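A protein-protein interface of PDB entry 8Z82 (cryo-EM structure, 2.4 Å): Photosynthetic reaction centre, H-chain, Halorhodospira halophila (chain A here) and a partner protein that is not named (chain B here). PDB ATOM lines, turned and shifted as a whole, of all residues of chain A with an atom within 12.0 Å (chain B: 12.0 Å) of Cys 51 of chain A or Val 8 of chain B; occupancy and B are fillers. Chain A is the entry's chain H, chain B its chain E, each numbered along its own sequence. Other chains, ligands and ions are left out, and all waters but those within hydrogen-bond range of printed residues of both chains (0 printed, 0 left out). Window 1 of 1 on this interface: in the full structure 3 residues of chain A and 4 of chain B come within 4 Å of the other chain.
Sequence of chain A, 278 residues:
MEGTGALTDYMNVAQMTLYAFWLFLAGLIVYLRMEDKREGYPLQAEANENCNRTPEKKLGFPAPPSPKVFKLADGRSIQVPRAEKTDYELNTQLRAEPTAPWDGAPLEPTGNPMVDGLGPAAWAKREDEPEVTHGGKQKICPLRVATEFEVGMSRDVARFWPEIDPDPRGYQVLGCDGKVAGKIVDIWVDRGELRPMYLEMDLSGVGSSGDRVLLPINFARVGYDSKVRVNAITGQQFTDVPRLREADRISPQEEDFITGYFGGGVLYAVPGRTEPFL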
ATOM      1  N   ALA A  45     -17.520  -6.314   8.185  1.00  0.00           N
ATOM      2  CA  ALA A  45     -18.204  -5.958   9.419  1.00  0.00           C
ATOM      3  C   ALA A  45     -19.007  -4.693   9.156  1.00  0.00           C
ATOM      4  O   ALA A  45     -18.435  -3.640   8.868  1.00  0.00           O
ATOM      5  CB  ALA A  45     -17.207  -5.750  10.553  1.00  0.00           C
ATOM      6  N   GLU A  46     -20.328  -4.795   9.237  1.00  0.00           N
ATOM      7  CA  GLU A  46     -21.158  -3.621   9.038  1.00  0.00           C
ATOM      8  C   GLU A  46     -21.068  -2.705  10.252  1.00  0.00           C
ATOM      9  O   GLU A  46     -20.552  -3.075  11.309  1.00  0.00           O
ATOM     10  CB  GLU A  46     -22.603  -4.028   8.768  1.00  0.00           C
ATOM     11  CG  GLU A  46     -22.763  -4.895   7.543  1.00  0.00           C
ATOM     12  CD  GLU A  46     -24.061  -4.629   6.813  1.00  0.00           C
ATOM     13  OE1 GLU A  46     -24.593  -3.509   6.941  1.00  0.00           O
ATOM     14  OE2 GLU A  46     -24.554  -5.544   6.120  1.00  0.00           O
ATOM     15  N   ALA A  47     -21.563  -1.478  10.080  1.00  0.00           N
ATOM     16  CA  ALA A  47     -21.518  -0.509  11.168  1.00  0.00           C
ATOM     17  C   ALA A  47     -22.332  -0.982  12.363  1.00  0.00           C
ATOM     18  O   ALA A  47     -21.918  -0.804  13.513  1.00  0.00           O
ATOM     19  CB  ALA A  47     -22.021   0.848  10.683  1.00  0.00           C
ATOM     20  N   ASN A  48     -23.491  -1.594  12.112  1.00  0.00           N
ATOM     21  CA  ASN A  48     -24.385  -1.987  13.194  1.00  0.00           C
ATOM     22  C   ASN A  48     -23.915  -3.227  13.946  1.00  0.00           C
ATOM     23  O   ASN A  48     -24.664  -3.736  14.785  1.00  0.00           O
ATOM     24  CB  ASN A  48     -25.801  -2.204  12.655  1.00  0.00           C
ATOM     25  CG  ASN A  48     -25.925  -3.452  11.817  1.00  0.00           C
ATOM     26  OD1 ASN A  48     -26.373  -4.487  12.297  1.00  0.00           O
ATOM     27  ND2 ASN A  48     -25.541  -3.360  10.553  1.00  0.00           N
ATOM     28  N   GLU A  49     -22.709  -3.721  13.678  1.00  0.00           N
ATOM     29  CA  GLU A  49     -22.137  -4.813  14.454  1.00  0.00           C
ATOM     30  C   GLU A  49     -21.103  -4.331  15.455  1.00  0.00           C
ATOM     31  O   GLU A  49     -20.803  -5.044  16.420  1.00  0.00           O
ATOM     32  CB  GLU A  49     -21.482  -5.841  13.533  1.00  0.00           C
ATOM     33  CG  GLU A  49     -22.270  -6.152  12.277  1.00  0.00           C
ATOM     34  CD  GLU A  49     -21.493  -7.024  11.325  1.00  0.00           C
ATOM     35  OE1 GLU A  49     -20.277  -7.186  11.548  1.00  0.00           O
ATOM     36  OE2 GLU A  49     -22.095  -7.557  10.367  1.00  0.00           O
ATOM     37  N   ASN A  50     -20.558  -3.139  15.247  1.00  0.00           N
ATOM     38  CA  ASN A  50     -19.421  -2.631  15.995  1.00  0.00           C
ATOM     39  C   ASN A  50     -19.845  -1.470  16.887  1.00  0.00           C
ATOM     40  O   ASN A  50     -20.661  -0.632  16.500  1.00  0.00           O
ATOM     41  CB  ASN A  50     -18.307  -2.186  15.043  1.00  0.00           C
ATOM     42  CG  ASN A  50     -17.840  -3.303  14.126  1.00  0.00           C
ATOM     43  OD1 ASN A  50     -18.177  -4.471  14.323  1.00  0.00           O
ATOM     44  ND2 ASN A  50     -17.048  -2.949  13.124  1.00  0.00           N
ATOM     45  N   CYS A  51     -19.272  -1.428  18.090  1.00  0.00           N
ATOM     46  CA  CYS A  51     -19.619  -0.396  19.060  1.00  0.00           C
ATOM     47  C   CYS A  51     -19.243   1.003  18.593  1.00  0.00           C
ATOM     48  O   CYS A  51     -19.804   1.980  19.098  1.00  0.00           O
ATOM     49  CB  CYS A  51     -18.943  -0.680  20.402  1.00  0.00           C
ATOM     50  SG  CYS A  51     -19.598  -2.094  21.299  1.00  0.00           S
ATOM     51  N   ASN A  52     -18.304   1.127  17.658  1.00  0.00           N
ATOM     52  CA  ASN A  52     -17.936   2.430  17.125  1.00  0.00           C
ATOM     53  C   ASN A  52     -18.805   2.855  15.952  1.00  0.00           C
ATOM     54  O   ASN A  52     -18.589   3.942  15.408  1.00  0.00           O
ATOM     55  CB  ASN A  52     -16.455   2.451  16.722  1.00  0.00           C
ATOM     56  CG  ASN A  52     -15.995   1.164  16.064  1.00  0.00           C
ATOM     57  OD1 ASN A  52     -16.785   0.425  15.491  1.00  0.00           O
ATOM     58  ND2 ASN A  52     -14.700   0.904  16.130  1.00  0.00           N
ATOM     59  N   ARG A  53     -19.783   2.034  15.572  1.00  0.00           N
ATOM     60  CA  ARG A  53     -20.725   2.351  14.501  1.00  0.00           C
ATOM     61  C   ARG A  53     -20.000   2.742  13.220  1.00  0.00           C
ATOM     62  O   ARG A  53     -20.367   3.704  12.544  1.00  0.00           O
ATOM     63  CB  ARG A  53     -21.700   3.449  14.928  1.00  0.00           C
ATOM     64  CG  ARG A  53     -22.795   2.970  15.856  1.00  0.00           C
ATOM     65  CD  ARG A  53     -22.682   3.610  17.225  1.00  0.00           C
ATOM     66  NE  ARG A  53     -22.484   5.052  17.135  1.00  0.00           N
ATOM     67  CZ  ARG A  53     -22.700   5.899  18.131  1.00  0.00           C
ATOM     68  NH1 ARG A  53     -23.147   5.485  19.306  1.00  0.00           N
ATOM     69  NH2 ARG A  53     -22.475   7.197  17.942  1.00  0.00           N
ATOM     70  N   THR A  54     -18.952   1.990  12.884  1.00  0.00           N
ATOM     71  CA  THR A  54     -18.231   2.177  11.637  1.00  0.00           C
ATOM     72  C   THR A  54     -18.032   0.828  10.959  1.00  0.00           C
ATOM     73  O   THR A  54     -17.749  -0.172  11.634  1.00  0.00           O
ATOM     74  CB  THR A  54     -16.869   2.859  11.855  1.00  0.00           C
ATOM     75  OG1 THR A  54     -16.133   2.870  10.627  1.00  0.00           O
ATOM     76  CG2 THR A  54     -16.073   2.133  12.902  1.00  0.00           C
ATOM     77  N   PRO A  55     -18.202   0.763   9.643  1.00  0.00           N
ATOM     78  CA  PRO A  55     -17.900  -0.478   8.924  1.00  0.00           C
ATOM     79  C   PRO A  55     -16.408  -0.763   8.943  1.00  0.00           C
ATOM     80  O   PRO A  55     -15.579   0.148   8.957  1.00  0.00           O
ATOM     81  CB  PRO A  55     -18.400  -0.201   7.501  1.00  0.00           C
ATOM     82  CG  PRO A  55     -19.337   0.954   7.640  1.00  0.00           C
ATOM     83  CD  PRO A  55     -18.828   1.772   8.776  1.00  0.00           C
ATOM     84  N   GLU A  56     -16.073  -2.052   8.954  1.00  0.00           N
ATOM     85  CA  GLU A  56     -14.697  -2.500   9.107  1.00  0.00           C
ATOM     86  C   GLU A  56     -14.495  -3.772   8.296  1.00  0.00           C
ATOM     87  O   GLU A  56     -15.405  -4.259   7.622  1.00  0.00           O
ATOM     88  CB  GLU A  56     -14.342  -2.740  10.581  1.00  0.00           C
ATOM     89  CG  GLU A  56     -14.377  -1.487  11.441  1.00  0.00           C
ATOM     90  CD  GLU A  56     -13.880  -1.714  12.851  1.00  0.00           C
ATOM     91  OE1 GLU A  56     -14.102  -2.812  13.399  1.00  0.00           O
ATOM     92  OE2 GLU A  56     -13.269  -0.785  13.416  1.00  0.00           O
ATOM     93  N   LYS A  57     -13.279  -4.303   8.362  1.00  0.00           N
ATOM     94  CA  LYS A  57     -12.932  -5.572   7.740  1.00  0.00           C
ATOM     95  C   LYS A  57     -12.266  -6.474   8.767  1.00  0.00           C
ATOM     96  O   LYS A  57     -11.330  -6.055   9.456  1.00  0.00           O
ATOM     97  CB  LYS A  57     -12.012  -5.366   6.534  1.00  0.00           C
ATOM     98  CG  LYS A  57     -12.763  -5.052   5.249  1.00  0.00           C
ATOM     99  CD  LYS A  57     -11.926  -4.245   4.276  1.00  0.00           C
ATOM    100  CE  LYS A  57     -12.543  -4.244   2.880  1.00  0.00           C
ATOM    101  NZ  LYS A  57     -13.920  -3.673   2.842  1.00  0.00           N
ATOM    102  N   LYS A  58     -12.753  -7.705   8.869  1.00  0.00           N
ATOM    103  CA  LYS A  58     -12.180  -8.715   9.741  1.00  0.00           C
ATOM    104  C   LYS A  58     -11.449  -9.739   8.890  1.00  0.00           C
ATOM    105  O   LYS A  58     -12.010 -10.258   7.922  1.00  0.00           O
ATOM    106  CB  LYS A  58     -13.257  -9.401  10.583  1.00  0.00           C
ATOM    107  CG  LYS A  58     -13.865  -8.528  11.653  1.00  0.00           C
ATOM    108  CD  LYS A  58     -14.756  -9.348  12.576  1.00  0.00           C
ATOM    109  CE  LYS A  58     -15.626  -8.464  13.454  1.00  0.00           C
ATOM    110  NZ  LYS A  58     -16.423  -9.274  14.415  1.00  0.00           N
ATOM    111  N   PRO A 101     -32.531  -3.470  13.509  1.00  0.00           N
ATOM    112  CA  PRO A 101     -31.247  -2.805  13.248  1.00  0.00           C
ATOM    113  C   PRO A 101     -30.032  -3.544  13.772  1.00  0.00           C
ATOM    114  O   PRO A 101     -28.924  -3.269  13.300  1.00  0.00           O
ATOM    115  CB  PRO A 101     -31.405  -1.448  13.945  1.00  0.00           C
ATOM    116  CG  PRO A 101     -32.487  -1.658  14.942  1.00  0.00           C
ATOM    117  CD  PRO A 101     -33.406  -2.681  14.387  1.00  0.00           C
ATOM    118  N   TRP A 102     -30.189  -4.467  14.715  1.00  0.00           N
ATOM    119  CA  TRP A 102     -29.022  -5.124  15.278  1.00  0.00           C
ATOM    120  C   TRP A 102     -28.417  -6.113  14.284  1.00  0.00           C
ATOM    121  O   TRP A 102     -29.067  -6.557  13.333  1.00  0.00           O
ATOM    122  CB  TRP A 102     -29.368  -5.824  16.593  1.00  0.00           C
ATOM    123  CG  TRP A 102     -30.721  -6.468  16.679  1.00  0.00           C
ATOM    124  CD1 TRP A 102     -31.875  -5.889  17.109  1.00  0.00           C
ATOM    125  CD2 TRP A 102     -31.044  -7.831  16.379  1.00  0.00           C
ATOM    126  NE1 TRP A 102     -32.898  -6.798  17.078  1.00  0.00           N
ATOM    127  CE2 TRP A 102     -32.415  -7.998  16.629  1.00  0.00           C
ATOM    128  CE3 TRP A 102     -30.308  -8.919  15.909  1.00  0.00           C
ATOM    129  CZ2 TRP A 102     -33.066  -9.213  16.431  1.00  0.00           C
ATOM    130  CZ3 TRP A 102     -30.956 -10.125  15.714  1.00  0.00           C
ATOM    131  CH2 TRP A 102     -32.317 -10.262  15.969  1.00  0.00           C
ATOM    132  N   ASP A 103     -27.146  -6.441  14.509  1.00  0.00           N
ATOM    133  CA  ASP A 103     -26.453  -7.382  13.641  1.00  0.00           C
ATOM    134  C   ASP A 103     -27.057  -8.770  13.763  1.00  0.00           C
ATOM    135  O   ASP A 103     -27.408  -9.220  14.854  1.00  0.00           O
ATOM    136  CB  ASP A 103     -24.964  -7.444  13.976  1.00  0.00           C
ATOM    137  CG  ASP A 103     -24.681  -8.184  15.275  1.00  0.00           C
ATOM    138  OD1 ASP A 103     -25.103  -7.700  16.342  1.00  0.00           O
ATOM    139  OD2 ASP A 103     -24.046  -9.260  15.225  1.00  0.00           O
ATOM    140  N   ASN B   7     -13.284   5.540  15.232  1.00  0.00           N
ATOM    141  CA  ASN B   7     -13.601   4.630  16.327  1.00  0.00           C
ATOM    142  C   ASN B   7     -14.555   5.279  17.322  1.00  0.00           C
ATOM    143  O   ASN B   7     -15.112   6.341  17.051  1.00  0.00           O
ATOM    144  CB  ASN B   7     -12.326   4.173  17.039  1.00  0.00           C
ATOM    145  CG  ASN B   7     -11.411   5.325  17.407  1.00  0.00           C
ATOM    146  OD1 ASN B   7     -11.837   6.474  17.511  1.00  0.00           O
ATOM    147  ND2 ASN B   7     -10.141   5.016  17.608  1.00  0.00           N
ATOM    148  N   VAL B   8     -14.748   4.628  18.471  1.00  0.00           N
ATOM    149  CA  VAL B   8     -15.566   5.217  19.521  1.00  0.00           C
ATOM    150  C   VAL B   8     -14.917   6.510  19.995  1.00  0.00           C
ATOM    151  O   VAL B   8     -13.690   6.664  19.974  1.00  0.00           O
ATOM    152  CB  VAL B   8     -15.769   4.245  20.700  1.00  0.00           C
ATOM    153  CG1 VAL B   8     -16.319   2.920  20.222  1.00  0.00           C
ATOM    154  CG2 VAL B   8     -14.475   4.034  21.457  1.00  0.00           C
ATOM    155  N   SER B   9     -15.747   7.454  20.414  1.00  0.00           N
ATOM    156  CA  SER B   9     -15.236   8.670  21.016  1.00  0.00           C
ATOM    157  C   SER B   9     -14.780   8.372  22.439  1.00  0.00           C
ATOM    158  O   SER B   9     -14.876   7.244  22.930  1.00  0.00           O
ATOM    159  CB  SER B   9     -16.295   9.770  20.986  1.00  0.00           C
ATOM    160  OG  SER B   9     -17.364   9.485  21.871  1.00  0.00           O
ATOM    161  N   ASP B  10     -14.252   9.392  23.107  1.00  0.00           N
ATOM    162  CA  ASP B  10     -13.878   9.228  24.506  1.00  0.00           C
ATOM    163  C   ASP B  10     -15.110   9.056  25.382  1.00  0.00           C
ATOM    164  O   ASP B  10     -15.096   8.264  26.329  1.00  0.00           O
ATOM    165  CB  ASP B  10     -13.046  10.420  24.973  1.00  0.00           C
ATOM    166  CG  ASP B  10     -11.794  10.614  24.147  1.00  0.00           C
ATOM    167  OD1 ASP B  10     -11.915  10.928  22.943  1.00  0.00           O
ATOM    168  OD2 ASP B  10     -10.688  10.455  24.698  1.00  0.00           O
ATOM    169  N   GLU B  11     -16.184   9.791  25.080  1.00  0.00           N
ATOM    170  CA  GLU B  11     -17.393   9.721  25.894  1.00  0.00           C
ATOM    171  C   GLU B  11     -18.062   8.356  25.797  1.00  0.00           C
ATOM    172  O   GLU B  11     -18.510   7.810  26.811  1.00  0.00           O
ATOM    173  CB  GLU B  11     -18.365  10.824  25.480  1.00  0.00           C
ATOM    174  CG  GLU B  11     -19.496  11.056  26.467  1.00  0.00           C
ATOM    175  CD  GLU B  11     -19.940  12.510  26.511  1.00  0.00           C
ATOM    176  OE1 GLU B  11     -20.739  12.922  25.646  1.00  0.00           O
ATOM    177  OE2 GLU B  11     -19.484  13.241  27.412  1.00  0.00           O
ATOM    178  N   GLU B  12     -18.159   7.795  24.588  1.00  0.00           N
ATOM    179  CA  GLU B  12     -18.704   6.448  24.446  1.00  0.00           C
ATOM    180  C   GLU B  12     -17.838   5.428  25.168  1.00  0.00           C
ATOM    181  O   GLU B  12     -18.355   4.542  25.858  1.00  0.00           O
ATOM    182  CB  GLU B  12     -18.833   6.078  22.967  1.00  0.00           C
ATOM    183  CG  GLU B  12     -20.259   6.032  22.423  1.00  0.00           C
ATOM    184  CD  GLU B  12     -21.059   4.835  22.926  1.00  0.00           C
ATOM    185  OE1 GLU B  12     -20.590   4.131  23.844  1.00  0.00           O
ATOM    186  OE2 GLU B  12     -22.168   4.600  22.401  1.00  0.00           O
ATOM    187  N   ALA B  13     -16.515   5.541  25.024  1.00  0.00           N
ATOM    188  CA  ALA B  13     -15.612   4.592  25.664  1.00  0.00           C
ATOM    189  C   ALA B  13     -15.634   4.739  27.178  1.00  0.00           C
ATOM    190  O   ALA B  13     -15.408   3.767  27.904  1.00  0.00           O
ATOM    191  CB  ALA B  13     -14.196   4.775  25.128  1.00  0.00           C
ATOM    192  N   LYS B  14     -15.888   5.950  27.677  1.00  0.00           N
ATOM    193  CA  LYS B  14     -16.001   6.141  29.117  1.00  0.00           C
ATOM    194  C   LYS B  14     -17.326   5.600  29.643  1.00  0.00           C
ATOM    195  O   LYS B  14     -17.396   5.114  30.777  1.00  0.00           O
ATOM    196  CB  LYS B  14     -15.822   7.619  29.468  1.00  0.00           C
ATOM    197  CG  LYS B  14     -14.367   8.052  29.465  1.00  0.00           C
ATOM    198  CD  LYS B  14     -14.190   9.555  29.551  1.00  0.00           C
ATOM    199  CE  LYS B  14     -12.747   9.938  29.261  1.00  0.00           C
ATOM    200  NZ  LYS B  14     -12.439  11.359  29.577  1.00  0.00           N
ATOM    201  N   GLU B  15     -18.386   5.669  28.837  1.00  0.00           N
ATOM    202  CA  GLU B  15     -19.641   5.037  29.232  1.00  0.00           C
ATOM    203  C   GLU B  15     -19.525   3.520  29.203  1.00  0.00           C
ATOM    204  O   GLU B  15     -20.148   2.832  30.018  1.00  0.00           O
ATOM    205  CB  GLU B  15     -20.777   5.505  28.330  1.00  0.00           C
ATOM    206  CG  GLU B  15     -21.146   6.957  28.520  1.00  0.00           C
ATOM    207  CD  GLU B  15     -21.950   7.504  27.364  1.00  0.00           C
ATOM    208  OE1 GLU B  15     -22.421   6.694  26.536  1.00  0.00           O
ATOM    209  OE2 GLU B  15     -22.113   8.740  27.286  1.00  0.00           O
ATOM    210  N   PHE B  16     -18.747   2.983  28.261  1.00  0.00           N
ATOM    211  CA  PHE B  16     -18.443   1.556  28.280  1.00  0.00           C
ATOM    212  C   PHE B  16     -17.733   1.169  29.568  1.00  0.00           C
ATOM    213  O   PHE B  16     -18.103   0.190  30.222  1.00  0.00           O
ATOM    214  CB  PHE B  16     -17.574   1.178  27.080  1.00  0.00           C
ATOM    215  CG  PHE B  16     -18.300   1.165  25.773  1.00  0.00           C
ATOM    216  CD1 PHE B  16     -19.676   1.090  25.723  1.00  0.00           C
ATOM    217  CD2 PHE B  16     -17.594   1.214  24.585  1.00  0.00           C
ATOM    218  CE1 PHE B  16     -20.330   1.072  24.517  1.00  0.00           C
ATOM    219  CE2 PHE B  16     -18.245   1.195  23.378  1.00  0.00           C
ATOM    220  CZ  PHE B  16     -19.613   1.126  23.343  1.00  0.00           C
ATOM    221  N   HIS B  17     -16.717   1.940  29.954  1.00  0.00           N
ATOM    222  CA  HIS B  17     -15.913   1.572  31.110  1.00  0.00           C
ATOM    223  C   HIS B  17     -16.647   1.831  32.417  1.00  0.00           C
ATOM    224  O   HIS B  17     -16.352   1.180  33.424  1.00  0.00           O
ATOM    225  CB  HIS B  17     -14.585   2.319  31.083  1.00  0.00           C
ATOM    226  CG  HIS B  17     -13.629   1.880  32.146  1.00  0.00           C
ATOM    227  ND1 HIS B  17     -12.954   0.681  32.089  1.00  0.00           N
ATOM    228  CD2 HIS B  17     -13.254   2.469  33.303  1.00  0.00           C
ATOM    229  CE1 HIS B  17     -12.193   0.557  33.160  1.00  0.00           C
ATOM    230  NE2 HIS B  17     -12.355   1.629  33.912  1.00  0.00           N
ATOM    231  N   ALA B  18     -17.591   2.771  32.437  1.00  0.00           N
ATOM    232  CA  ALA B  18     -18.406   2.947  33.632  1.00  0.00           C
ATOM    233  C   ALA B  18     -19.275   1.723  33.881  1.00  0.00           C
ATOM    234  O   ALA B  18     -19.376   1.245  35.015  1.00  0.00           O
ATOM    235  CB  ALA B  18     -19.267   4.201  33.511  1.00  0.00           C
ATOM    236  N   MET B  19     -19.902   1.201  32.826  1.00  0.00           N
ATOM    237  CA  MET B  19     -20.686  -0.022  32.953  1.00  0.00           C
ATOM    238  C   MET B  19     -19.801  -1.204  33.315  1.00  0.00           C
ATOM    239  O   MET B  19     -20.199  -2.071  34.100  1.00  0.00           O
ATOM    240  CB  MET B  19     -21.433  -0.296  31.651  1.00  0.00           C
ATOM    241  CG  MET B  19     -22.573   0.661  31.375  1.00  0.00           C
ATOM    242  SD  MET B  19     -23.120   0.590  29.663  1.00  0.00           S
ATOM    243  CE  MET B  19     -23.371  -1.167  29.487  1.00  0.00           C
ATOM    244  N   PHE B  20     -18.599  -1.259  32.740  1.00  0.00           N
ATOM    245  CA  PHE B  20     -17.669  -2.338  33.048  1.00  0.00           C
ATOM    246  C   PHE B  20     -17.201  -2.278  34.493  1.00  0.00           C
ATOM    247  O   PHE B  20     -17.134  -3.307  35.171  1.00  0.00           O
ATOM    248  CB  PHE B  20     -16.473  -2.278  32.104  1.00  0.00           C
ATOM    249  CG  PHE B  20     -15.300  -3.100  32.554  1.00  0.00           C
ATOM    250  CD1 PHE B  20     -15.210  -4.436  32.215  1.00  0.00           C
ATOM    251  CD2 PHE B  20     -14.280  -2.535  33.306  1.00  0.00           C
ATOM    252  CE1 PHE B  20     -14.136  -5.192  32.621  1.00  0.00           C
ATOM    253  CE2 PHE B  20     -13.205  -3.291  33.715  1.00  0.00           C
ATOM    254  CZ  PHE B  20     -13.135  -4.620  33.370  1.00  0.00           C
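OE2 of Glu 12 of chain B lies within salt-bridge range of NH1 of Arg 53 of chain A (3.4 Å).
O of Cys 51 of chain A touches CG1 of Val 8 of chain B (3.8 Å).
Cys 51 of chain A touches Phe 16 of chain B.
Asn 7 of chain B touches Asn 52 of chain A.
Val 8 of chain B touches Asn 52 of chain A.
Of the printed residues of chain B, Cys 51 of chain A touches Val 8 and Phe 16.
Of chain A, only Cys 51 (3.8 Å) and Asn 52 (3.3 Å) come within 4 Å of Val 8 of chain B.
Of chain B, only Asn 7 and Val 8 come within 4 Å of Asn 52 of chain A.
Arg 53 of chain A touches one residue of chain B.
Ser 9 of chain B touches none of the printed residues of chain A.
No residue of chain A comes within 4 Å of Asp 10 of chain B.
No residue of chain A comes within 4 Å of Ala 13 of chain B.
Printed residues of chain A within 4 Å of Phe 16 of chain B: Cys 51 (3.5 Å).
Lys 14 of chain B touches none of the printed residues of chain A.
Met 19 of chain B touches none of the printed residues of chain A.
The nearest residue of chain A that does not touch Val 8 of chain B is Arg 53 of chain A (5.9 Å).
The nearest printed residue of chain A that does not touch Phe 16 of chain B is Asn 52 of chain A (5.7 Å).
Of the 17 printed residues of chain A, 3 touch a printed residue of chain B.
Printed residues of chain A that touch a printed residue of chain B: Cys 51, Asn 52 and Arg 53.
Along chain A the printed residues that touch a printed residue of chain B span positions 51 to 53.
OG of Ser 9 of chain B lies within hydrogen-bond range of N of Glu 12 of chain B (3.3 Å).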
